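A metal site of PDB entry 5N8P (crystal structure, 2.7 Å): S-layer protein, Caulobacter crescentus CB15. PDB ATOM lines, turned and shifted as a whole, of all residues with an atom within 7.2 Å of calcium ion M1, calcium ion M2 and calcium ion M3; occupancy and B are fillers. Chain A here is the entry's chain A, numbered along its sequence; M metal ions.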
ATOM      1  N   SER A 844       0.114   5.422  19.869  1.00  0.00           N
ATOM      2  CA  SER A 844      -1.241   5.977  19.909  1.00  0.00           C
ATOM      3  C   SER A 844      -1.449   7.126  18.867  1.00  0.00           C
ATOM      4  O   SER A 844      -1.491   8.345  19.163  1.00  0.00           O
ATOM      5  CB  SER A 844      -1.773   6.283  21.342  1.00  0.00           C
ATOM      6  OG  SER A 844      -0.835   6.539  22.368  1.00  0.00           O
ATOM      7  N   VAL A 846      -2.716   9.668  16.167  1.00  0.00           N
ATOM      8  CA  VAL A 846      -3.879  10.526  15.991  1.00  0.00           C
ATOM      9  C   VAL A 846      -3.960  11.044  14.566  1.00  0.00           C
ATOM     10  O   VAL A 846      -2.990  11.569  14.047  1.00  0.00           O
ATOM     11  CB  VAL A 846      -3.845  11.664  17.021  1.00  0.00           C
ATOM     12  CG1 VAL A 846      -4.970  12.665  16.779  1.00  0.00           C
ATOM     13  CG2 VAL A 846      -3.870  11.096  18.451  1.00  0.00           C
ATOM     14  N   ARG A 862      -2.666  20.160  17.524  1.00  0.00           N
ATOM     15  CA  ARG A 862      -1.663  19.513  18.388  1.00  0.00           C
ATOM     16  C   ARG A 862      -1.694  17.976  18.359  1.00  0.00           C
ATOM     17  O   ARG A 862      -2.695  17.390  18.731  1.00  0.00           O
ATOM     18  CB  ARG A 862      -1.841  19.997  19.834  1.00  0.00           C
ATOM     19  CG  ARG A 862      -0.654  20.708  20.423  1.00  0.00           C
ATOM     20  CD  ARG A 862      -0.798  22.185  20.190  1.00  0.00           C
ATOM     21  NE  ARG A 862      -1.703  22.899  21.114  1.00  0.00           N
ATOM     22  CZ  ARG A 862      -1.289  23.663  22.135  1.00  0.00           C
ATOM     23  NH1 ARG A 862      -2.172  24.227  22.934  1.00  0.00           N
ATOM     24  NH2 ARG A 862       0.009  23.895  22.348  1.00  0.00           N
ATOM     25  N   GLY A 863      -0.607  17.342  17.965  1.00  0.00           N
ATOM     26  CA  GLY A 863      -0.430  15.888  18.037  1.00  0.00           C
ATOM     27  C   GLY A 863       0.042  15.389  19.403  1.00  0.00           C
ATOM     28  O   GLY A 863       0.354  16.175  20.314  1.00  0.00           O
ATOM     29  N   GLY A 864       0.083  14.062  19.547  1.00  0.00           N
ATOM     30  CA  GLY A 864       0.465  13.399  20.795  1.00  0.00           C
ATOM     31  C   GLY A 864       1.729  12.589  20.661  1.00  0.00           C
ATOM     32  O   GLY A 864       2.556  12.883  19.801  1.00  0.00           O
ATOM     33  N   ALA A 865       1.920  11.593  21.510  1.00  0.00           N
ATOM     34  CA  ALA A 865       3.135  10.771  21.454  1.00  0.00           C
ATOM     35  C   ALA A 865       3.199   9.866  20.195  1.00  0.00           C
ATOM     36  O   ALA A 865       4.268   9.399  19.815  1.00  0.00           O
ATOM     37  CB  ALA A 865       3.319   9.986  22.725  1.00  0.00           C
ATOM     38  N   GLY A 866       2.072   9.654  19.527  1.00  0.00           N
ATOM     39  CA  GLY A 866       1.980   8.725  18.393  1.00  0.00           C
ATOM     40  C   GLY A 866       2.476   9.300  17.089  1.00  0.00           C
ATOM     41  O   GLY A 866       2.757  10.470  16.989  1.00  0.00           O
ATOM     42  N   ALA A 867       2.596   8.424  16.106  1.00  0.00           N
ATOM     43  CA  ALA A 867       2.985   8.828  14.743  1.00  0.00           C
ATOM     44  C   ALA A 867       1.746   9.468  14.102  1.00  0.00           C
ATOM     45  O   ALA A 867       0.964   8.764  13.432  1.00  0.00           O
ATOM     46  CB  ALA A 867       3.477   7.610  13.935  1.00  0.00           C
ATOM     47  N   ASP A 868       1.565  10.774  14.312  1.00  0.00           N
ATOM     48  CA  ASP A 868       0.280  11.448  13.989  1.00  0.00           C
ATOM     49  C   ASP A 868       0.196  11.994  12.546  1.00  0.00           C
ATOM     50  O   ASP A 868       1.211  12.210  11.886  1.00  0.00           O
ATOM     51  CB  ASP A 868      -0.044  12.569  14.986  1.00  0.00           C
ATOM     52  CG  ASP A 868       0.133  12.142  16.451  1.00  0.00           C
ATOM     53  OD1 ASP A 868      -0.506  11.174  16.969  1.00  0.00           O
ATOM     54  OD2 ASP A 868       0.940  12.802  17.116  1.00  0.00           O
ATOM     55  N   SER A 869      -1.033  12.230  12.070  1.00  0.00           N
ATOM     56  CA  SER A 869      -1.248  12.718  10.714  1.00  0.00           C
ATOM     57  C   SER A 869      -2.222  13.902  10.677  1.00  0.00           C
ATOM     58  O   SER A 869      -3.446  13.749  10.543  1.00  0.00           O
ATOM     59  CB  SER A 869      -1.679  11.588   9.781  1.00  0.00           C
ATOM     60  OG  SER A 869      -1.971  12.107   8.497  1.00  0.00           O
ATOM     61  N   LEU A 870      -1.631  15.088  10.757  1.00  0.00           N
ATOM     62  CA  LEU A 870      -2.337  16.321  10.986  1.00  0.00           C
ATOM     63  C   LEU A 870      -2.369  17.188   9.723  1.00  0.00           C
ATOM     64  O   LEU A 870      -1.316  17.588   9.218  1.00  0.00           O
ATOM     65  CB  LEU A 870      -1.661  17.044  12.160  1.00  0.00           C
ATOM     66  CG  LEU A 870      -1.262  16.187  13.381  1.00  0.00           C
ATOM     67  CD1 LEU A 870      -0.411  16.947  14.359  1.00  0.00           C
ATOM     68  CD2 LEU A 870      -2.471  15.608  14.083  1.00  0.00           C
ATOM     69  N   ILE A 881       1.485  21.144  15.433  1.00  0.00           N
ATOM     70  CA  ILE A 881       2.564  20.661  16.302  1.00  0.00           C
ATOM     71  C   ILE A 881       2.388  19.161  16.559  1.00  0.00           C
ATOM     72  O   ILE A 881       1.472  18.796  17.278  1.00  0.00           O
ATOM     73  CB  ILE A 881       2.587  21.431  17.651  1.00  0.00           C
ATOM     74  CG1 ILE A 881       3.027  22.872  17.435  1.00  0.00           C
ATOM     75  CG2 ILE A 881       3.467  20.796  18.718  1.00  0.00           C
ATOM     76  CD1 ILE A 881       2.305  23.889  18.261  1.00  0.00           C
ATOM     77  N   GLY A 882       3.220  18.298  15.975  1.00  0.00           N
ATOM     78  CA  GLY A 882       3.277  16.853  16.377  1.00  0.00           C
ATOM     79  C   GLY A 882       3.973  16.704  17.730  1.00  0.00           C
ATOM     80  O   GLY A 882       4.632  17.619  18.204  1.00  0.00           O
ATOM     81  N   GLY A 883       3.858  15.570  18.376  1.00  0.00           N
ATOM     82  CA  GLY A 883       4.568  15.418  19.673  1.00  0.00           C
ATOM     83  C   GLY A 883       5.899  14.725  19.526  1.00  0.00           C
ATOM     84  O   GLY A 883       6.787  15.200  18.838  1.00  0.00           O
ATOM     85  N   ALA A 884       6.023  13.583  20.205  1.00  0.00           N
ATOM     86  CA  ALA A 884       7.036  12.573  19.904  1.00  0.00           C
ATOM     87  C   ALA A 884       6.647  11.877  18.586  1.00  0.00           C
ATOM     88  O   ALA A 884       5.595  12.206  18.015  1.00  0.00           O
ATOM     89  CB  ALA A 884       7.182  11.587  21.067  1.00  0.00           C
ATOM     90  N   GLY A 885       7.498  10.962  18.063  1.00  0.00           N
ATOM     91  CA  GLY A 885       7.100  10.073  16.955  1.00  0.00           C
ATOM     92  C   GLY A 885       6.973  10.660  15.554  1.00  0.00           C
ATOM     93  O   GLY A 885       7.010  11.873  15.359  1.00  0.00           O
ATOM     94  N   ALA A 886       6.828   9.770  14.580  1.00  0.00           N
ATOM     95  CA  ALA A 886       6.938  10.092  13.141  1.00  0.00           C
ATOM     96  C   ALA A 886       5.698  10.841  12.589  1.00  0.00           C
ATOM     97  O   ALA A 886       4.820  10.239  11.956  1.00  0.00           O
ATOM     98  CB  ALA A 886       7.241   8.814  12.316  1.00  0.00           C
ATOM     99  N   ASP A 887       5.641  12.148  12.834  1.00  0.00           N
ATOM    100  CA  ASP A 887       4.462  12.933  12.491  1.00  0.00           C
ATOM    101  C   ASP A 887       4.474  13.366  11.045  1.00  0.00           C
ATOM    102  O   ASP A 887       5.542  13.631  10.487  1.00  0.00           O
ATOM    103  CB  ASP A 887       4.336  14.143  13.400  1.00  0.00           C
ATOM    104  CG  ASP A 887       4.231  13.771  14.860  1.00  0.00           C
ATOM    105  OD1 ASP A 887       3.267  13.041  15.209  1.00  0.00           O
ATOM    106  OD2 ASP A 887       5.082  14.203  15.659  1.00  0.00           O
ATOM    107  N   THR A 888       3.291  13.381  10.427  1.00  0.00           N
ATOM    108  CA  THR A 888       3.094  13.961   9.095  1.00  0.00           C
ATOM    109  C   THR A 888       2.244  15.238   9.238  1.00  0.00           C
ATOM    110  O   THR A 888       1.103  15.170   9.709  1.00  0.00           O
ATOM    111  CB  THR A 888       2.509  12.927   8.087  1.00  0.00           C
ATOM    112  OG1 THR A 888       3.406  11.817   7.963  1.00  0.00           O
ATOM    113  CG2 THR A 888       2.305  13.545   6.663  1.00  0.00           C
ATOM    114  N   LEU A 889       2.827  16.376   8.869  1.00  0.00           N
ATOM    115  CA  LEU A 889       2.171  17.672   8.943  1.00  0.00           C
ATOM    116  C   LEU A 889       1.920  18.142   7.525  1.00  0.00           C
ATOM    117  O   LEU A 889       2.848  18.259   6.741  1.00  0.00           O
ATOM    118  CB  LEU A 889       3.080  18.645   9.685  1.00  0.00           C
ATOM    119  CG  LEU A 889       3.139  18.584  11.219  1.00  0.00           C
ATOM    120  CD1 LEU A 889       3.683  17.283  11.772  1.00  0.00           C
ATOM    121  CD2 LEU A 889       3.965  19.738  11.752  1.00  0.00           C
ATOM    122  N   THR A 899       5.742  22.526  13.544  1.00  0.00           N
ATOM    123  CA  THR A 899       6.703  22.041  14.513  1.00  0.00           C
ATOM    124  C   THR A 899       6.429  20.554  14.640  1.00  0.00           C
ATOM    125  O   THR A 899       5.437  20.167  15.245  1.00  0.00           O
ATOM    126  CB  THR A 899       6.521  22.756  15.879  1.00  0.00           C
ATOM    127  OG1 THR A 899       6.591  24.178  15.708  1.00  0.00           O
ATOM    128  CG2 THR A 899       7.542  22.293  16.913  1.00  0.00           C
ATOM    129  N   GLY A 900       7.248  19.725  14.008  1.00  0.00           N
ATOM    130  CA  GLY A 900       7.197  18.284  14.307  1.00  0.00           C
ATOM    131  C   GLY A 900       8.163  18.223  15.450  1.00  0.00           C
ATOM    132  O   GLY A 900       9.245  18.780  15.310  1.00  0.00           O
ATOM    133  N   GLY A 901       7.820  17.623  16.579  1.00  0.00           N
ATOM    134  CA  GLY A 901       8.717  17.627  17.742  1.00  0.00           C
ATOM    135  C   GLY A 901       9.901  16.690  17.542  1.00  0.00           C
ATOM    136  O   GLY A 901      10.607  16.728  16.521  1.00  0.00           O
ATOM    137  N   THR A 902      10.110  15.834  18.530  1.00  0.00           N
ATOM    138  CA  THR A 902      11.105  14.774  18.426  1.00  0.00           C
ATOM    139  C   THR A 902      10.671  13.766  17.324  1.00  0.00           C
ATOM    140  O   THR A 902       9.479  13.706  16.970  1.00  0.00           O
ATOM    141  CB  THR A 902      11.324  14.099  19.798  1.00  0.00           C
ATOM    142  OG1 THR A 902      10.221  13.225  20.098  1.00  0.00           O
ATOM    143  CG2 THR A 902      11.440  15.142  20.929  1.00  0.00           C
ATOM    144  N   GLY A 903      11.645  13.030  16.771  1.00  0.00           N
ATOM    145  CA  GLY A 903      11.361  11.985  15.783  1.00  0.00           C
ATOM    146  C   GLY A 903      11.450  12.398  14.326  1.00  0.00           C
ATOM    147  O   GLY A 903      11.515  13.581  14.006  1.00  0.00           O
ATOM    148  N   ALA A 904      11.465  11.392  13.442  1.00  0.00           N
ATOM    149  CA  ALA A 904      11.583  11.575  11.996  1.00  0.00           C
ATOM    150  C   ALA A 904      10.272  12.096  11.422  1.00  0.00           C
ATOM    151  O   ALA A 904       9.448  11.319  10.918  1.00  0.00           O
ATOM    152  CB  ALA A 904      11.980  10.240  11.334  1.00  0.00           C
ATOM    153  N   ASP A 905      10.058  13.414  11.499  1.00  0.00           N
ATOM    154  CA  ASP A 905       8.807  14.002  11.022  1.00  0.00           C
ATOM    155  C   ASP A 905       8.826  14.225   9.523  1.00  0.00           C
ATOM    156  O   ASP A 905       9.893  14.409   8.955  1.00  0.00           O
ATOM    157  CB  ASP A 905       8.514  15.304  11.764  1.00  0.00           C
ATOM    158  CG  ASP A 905       8.473  15.110  13.260  1.00  0.00           C
ATOM    159  OD1 ASP A 905       7.534  14.454  13.753  1.00  0.00           O
ATOM    160  OD2 ASP A 905       9.381  15.614  13.932  1.00  0.00           O
ATOM    161  N   ILE A 906       7.670  14.147   8.891  1.00  0.00           N
ATOM    162  CA  ILE A 906       7.602  14.432   7.449  1.00  0.00           C
ATOM    163  C   ILE A 906       6.705  15.676   7.210  1.00  0.00           C
ATOM    164  O   ILE A 906       5.562  15.721   7.651  1.00  0.00           O
ATOM    165  CB  ILE A 906       7.401  13.138   6.539  1.00  0.00           C
ATOM    166  CG1 ILE A 906       6.325  13.324   5.419  1.00  0.00           C
ATOM    167  CG2 ILE A 906       7.250  11.832   7.363  1.00  0.00           C
ATOM    168  CD1 ILE A 906       6.127  12.128   4.472  1.00  0.00           C
ATOM    169  N   PHE A 907       7.278  16.725   6.601  1.00  0.00           N
ATOM    170  CA  PHE A 907       6.529  17.951   6.302  1.00  0.00           C
ATOM    171  C   PHE A 907       6.043  17.864   4.869  1.00  0.00           C
ATOM    172  O   PHE A 907       6.804  18.148   3.941  1.00  0.00           O
ATOM    173  CB  PHE A 907       7.383  19.184   6.535  1.00  0.00           C
ATOM    174  CG  PHE A 907       7.931  19.253   7.916  1.00  0.00           C
ATOM    175  CD1 PHE A 907       7.124  19.626   8.991  1.00  0.00           C
ATOM    176  CD2 PHE A 907       9.255  18.911   8.177  1.00  0.00           C
ATOM    177  CE1 PHE A 907       7.617  19.694  10.280  1.00  0.00           C
ATOM    178  CE2 PHE A 907       9.766  18.965   9.475  1.00  0.00           C
ATOM    179  CZ  PHE A 907       8.941  19.352  10.540  1.00  0.00           C
ATOM    180  N   ASP A 923      11.444  23.865  13.490  1.00  0.00           N
ATOM    181  CA  ASP A 923      12.487  23.034  14.118  1.00  0.00           C
ATOM    182  C   ASP A 923      13.097  21.937  13.263  1.00  0.00           C
ATOM    183  O   ASP A 923      13.581  20.922  13.809  1.00  0.00           O
ATOM    184  CB  ASP A 923      11.952  22.437  15.447  1.00  0.00           C
ATOM    185  CG  ASP A 923      10.808  21.419  15.244  1.00  0.00           C
ATOM    186  OD1 ASP A 923      10.307  21.154  14.093  1.00  0.00           O
ATOM    187  OD2 ASP A 923      10.417  20.887  16.292  1.00  0.00           O
ATOM    188  N   ALA A 924      13.061  22.129  11.944  1.00  0.00           N
ATOM    189  CA  ALA A 924      13.708  21.208  10.993  1.00  0.00           C
ATOM    190  C   ALA A 924      15.101  20.778  11.493  1.00  0.00           C
ATOM    191  O   ALA A 924      15.945  21.608  11.810  1.00  0.00           O
ATOM    192  CB  ALA A 924      13.796  21.838   9.617  1.00  0.00           C
ATOM    193  N   ALA A 925      15.270  19.479  11.622  1.00  0.00           N
ATOM    194  CA  ALA A 925      16.497  18.889  12.168  1.00  0.00           C
ATOM    195  C   ALA A 925      16.842  17.617  11.406  1.00  0.00           C
ATOM    196  O   ALA A 925      16.054  17.132  10.586  1.00  0.00           O
ATOM    197  CB  ALA A 925      16.357  18.609  13.666  1.00  0.00           C
ATOM    198  N   VAL A 926      18.048  17.115  11.660  1.00  0.00           N
ATOM    199  CA  VAL A 926      18.538  15.877  11.090  1.00  0.00           C
ATOM    200  C   VAL A 926      17.518  14.726  11.285  1.00  0.00           C
ATOM    201  O   VAL A 926      17.083  14.439  12.417  1.00  0.00           O
ATOM    202  CB  VAL A 926      19.961  15.563  11.638  1.00  0.00           C
ATOM    203  CG1 VAL A 926      19.985  15.438  13.175  1.00  0.00           C
ATOM    204  CG2 VAL A 926      20.574  14.343  10.951  1.00  0.00           C
ATOM    205  N   GLY A 927      17.111  14.117  10.170  1.00  0.00           N
ATOM    206  CA  GLY A 927      16.141  13.009  10.184  1.00  0.00           C
ATOM    207  C   GLY A 927      14.760  13.350   9.631  1.00  0.00           C
ATOM    208  O   GLY A 927      14.119  12.498   9.000  1.00  0.00           O
ATOM    209  N   ASP A 928      14.329  14.589   9.871  1.00  0.00           N
ATOM    210  CA  ASP A 928      13.084  15.111   9.304  1.00  0.00           C
ATOM    211  C   ASP A 928      13.129  15.161   7.781  1.00  0.00           C
ATOM    212  O   ASP A 928      14.215  15.313   7.206  1.00  0.00           O
ATOM    213  CB  ASP A 928      12.751  16.496   9.886  1.00  0.00           C
ATOM    214  CG  ASP A 928      12.491  16.478  11.406  1.00  0.00           C
ATOM    215  OD1 ASP A 928      12.933  17.406  12.114  1.00  0.00           O
ATOM    216  OD2 ASP A 928      11.837  15.551  11.927  1.00  0.00           O
HETATM  217 CA    CA M   1       3.234  12.892  17.441  1.00  0.00          CA
HETATM  218 CA    CA M   2       7.279  14.516  16.243  1.00  0.00          CA
HETATM  219 CA    CA M   3      11.643  15.998  14.368  1.00  0.00          CA
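C of Gly 882 touches calcium ion M1, 3.9 Å away. Of the 35 residues printed, 7 come within 4 Å of calcium ion M1. The nearest printed residue that does not touch calcium ion M1 is Ala 865 (4.1 Å).
C of Gly 900 touches calcium ion M2, at 3.9 Å. Eight residues have an atom within 4 Å of calcium ion M2: Gly 883, Ala 884, Gly 885, Asp 887, Gly 900, Gly 901, Thr 902 and Asp 905.
The backbone carbonyl oxygen (O) of Asp 887 lies within hydrogen-bond range of the backbone NH (N) of Ile 906, at 2.7 Å. The backbone NH (N) of Val 846 lies within hydrogen-bond range of the side-chain carboxylate (OD1) of Asp 868 (2.8 Å). The backbone carbonyl oxygen (O) of Asp 868 is in hydrogen-bond range of the backbone NH (N) of Thr 888, at 2.8 Å. N of Gly 883 lies close to O of Gly 864, at 3.3 Å. The side-chain carboxylate (OD1) of Asp 928 sits at hydrogen-bond distance from the backbone NH (N) of Ala 925, 3.2 Å away. The backbone carbonyl oxygen (O) of Gly 883 sits close to the backbone NH (N) of Gly 901, 3.5 Å away. OD1 of Asp 923 is in hydrogen-bond range of N of Gly 900, at 3.4 Å. The backbone carbonyl oxygen (O) of Thr 899 is in hydrogen-bond range of the backbone NH (N) of Gly 882.
Calcium ion M2 is bound by OD2 of Asp 887, O of Thr 902, OD1 of Asp 905, O of Gly 883 and O of Gly 885.
Calcium ion M1 is bound by OD1 of Asp 887 (2.2 Å). OD2 of Asp 868 is bound to calcium ion M1. O of Gly 864 binds calcium ion M1. O of Gly 866 is bound to calcium ion M1 (2.5 Å). The backbone carbonyl oxygen (O) of Ala 884 is bound to calcium ion M1, 2.5 Å away. The side-chain carboxylate (OD2) of Asp 887 is bound to calcium ion M1, at 2.9 Å. Calcium ion M1 has six donor atoms within binding distance. Slightly farther from calcium ion M1 lies N of Gly 883 (2.9 Å).
Residues that only touch calcium ion M3: Gly 900 (3.8 Å). Of the 35 residues printed, 6 come within 4 Å of calcium ion M3. The nearest printed residue that does not touch calcium ion M3 is Ala 904 (4.7 Å).
OD2 of Asp 905 is bound to calcium ion M3, at 2.3 Å. The backbone carbonyl oxygen (O) of Gly 903 is bound to calcium ion M3, at 2.4 Å. OD2 of Asp 928 is bound to calcium ion M3 (2.5 Å). The backbone carbonyl oxygen (O) of Gly 901 binds calcium ion M3 (2.5 Å). Calcium ion M3 has four donor atoms within binding distance. Slightly farther from calcium ion M3 lies OD1 of Asp 928 (3.0 Å).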
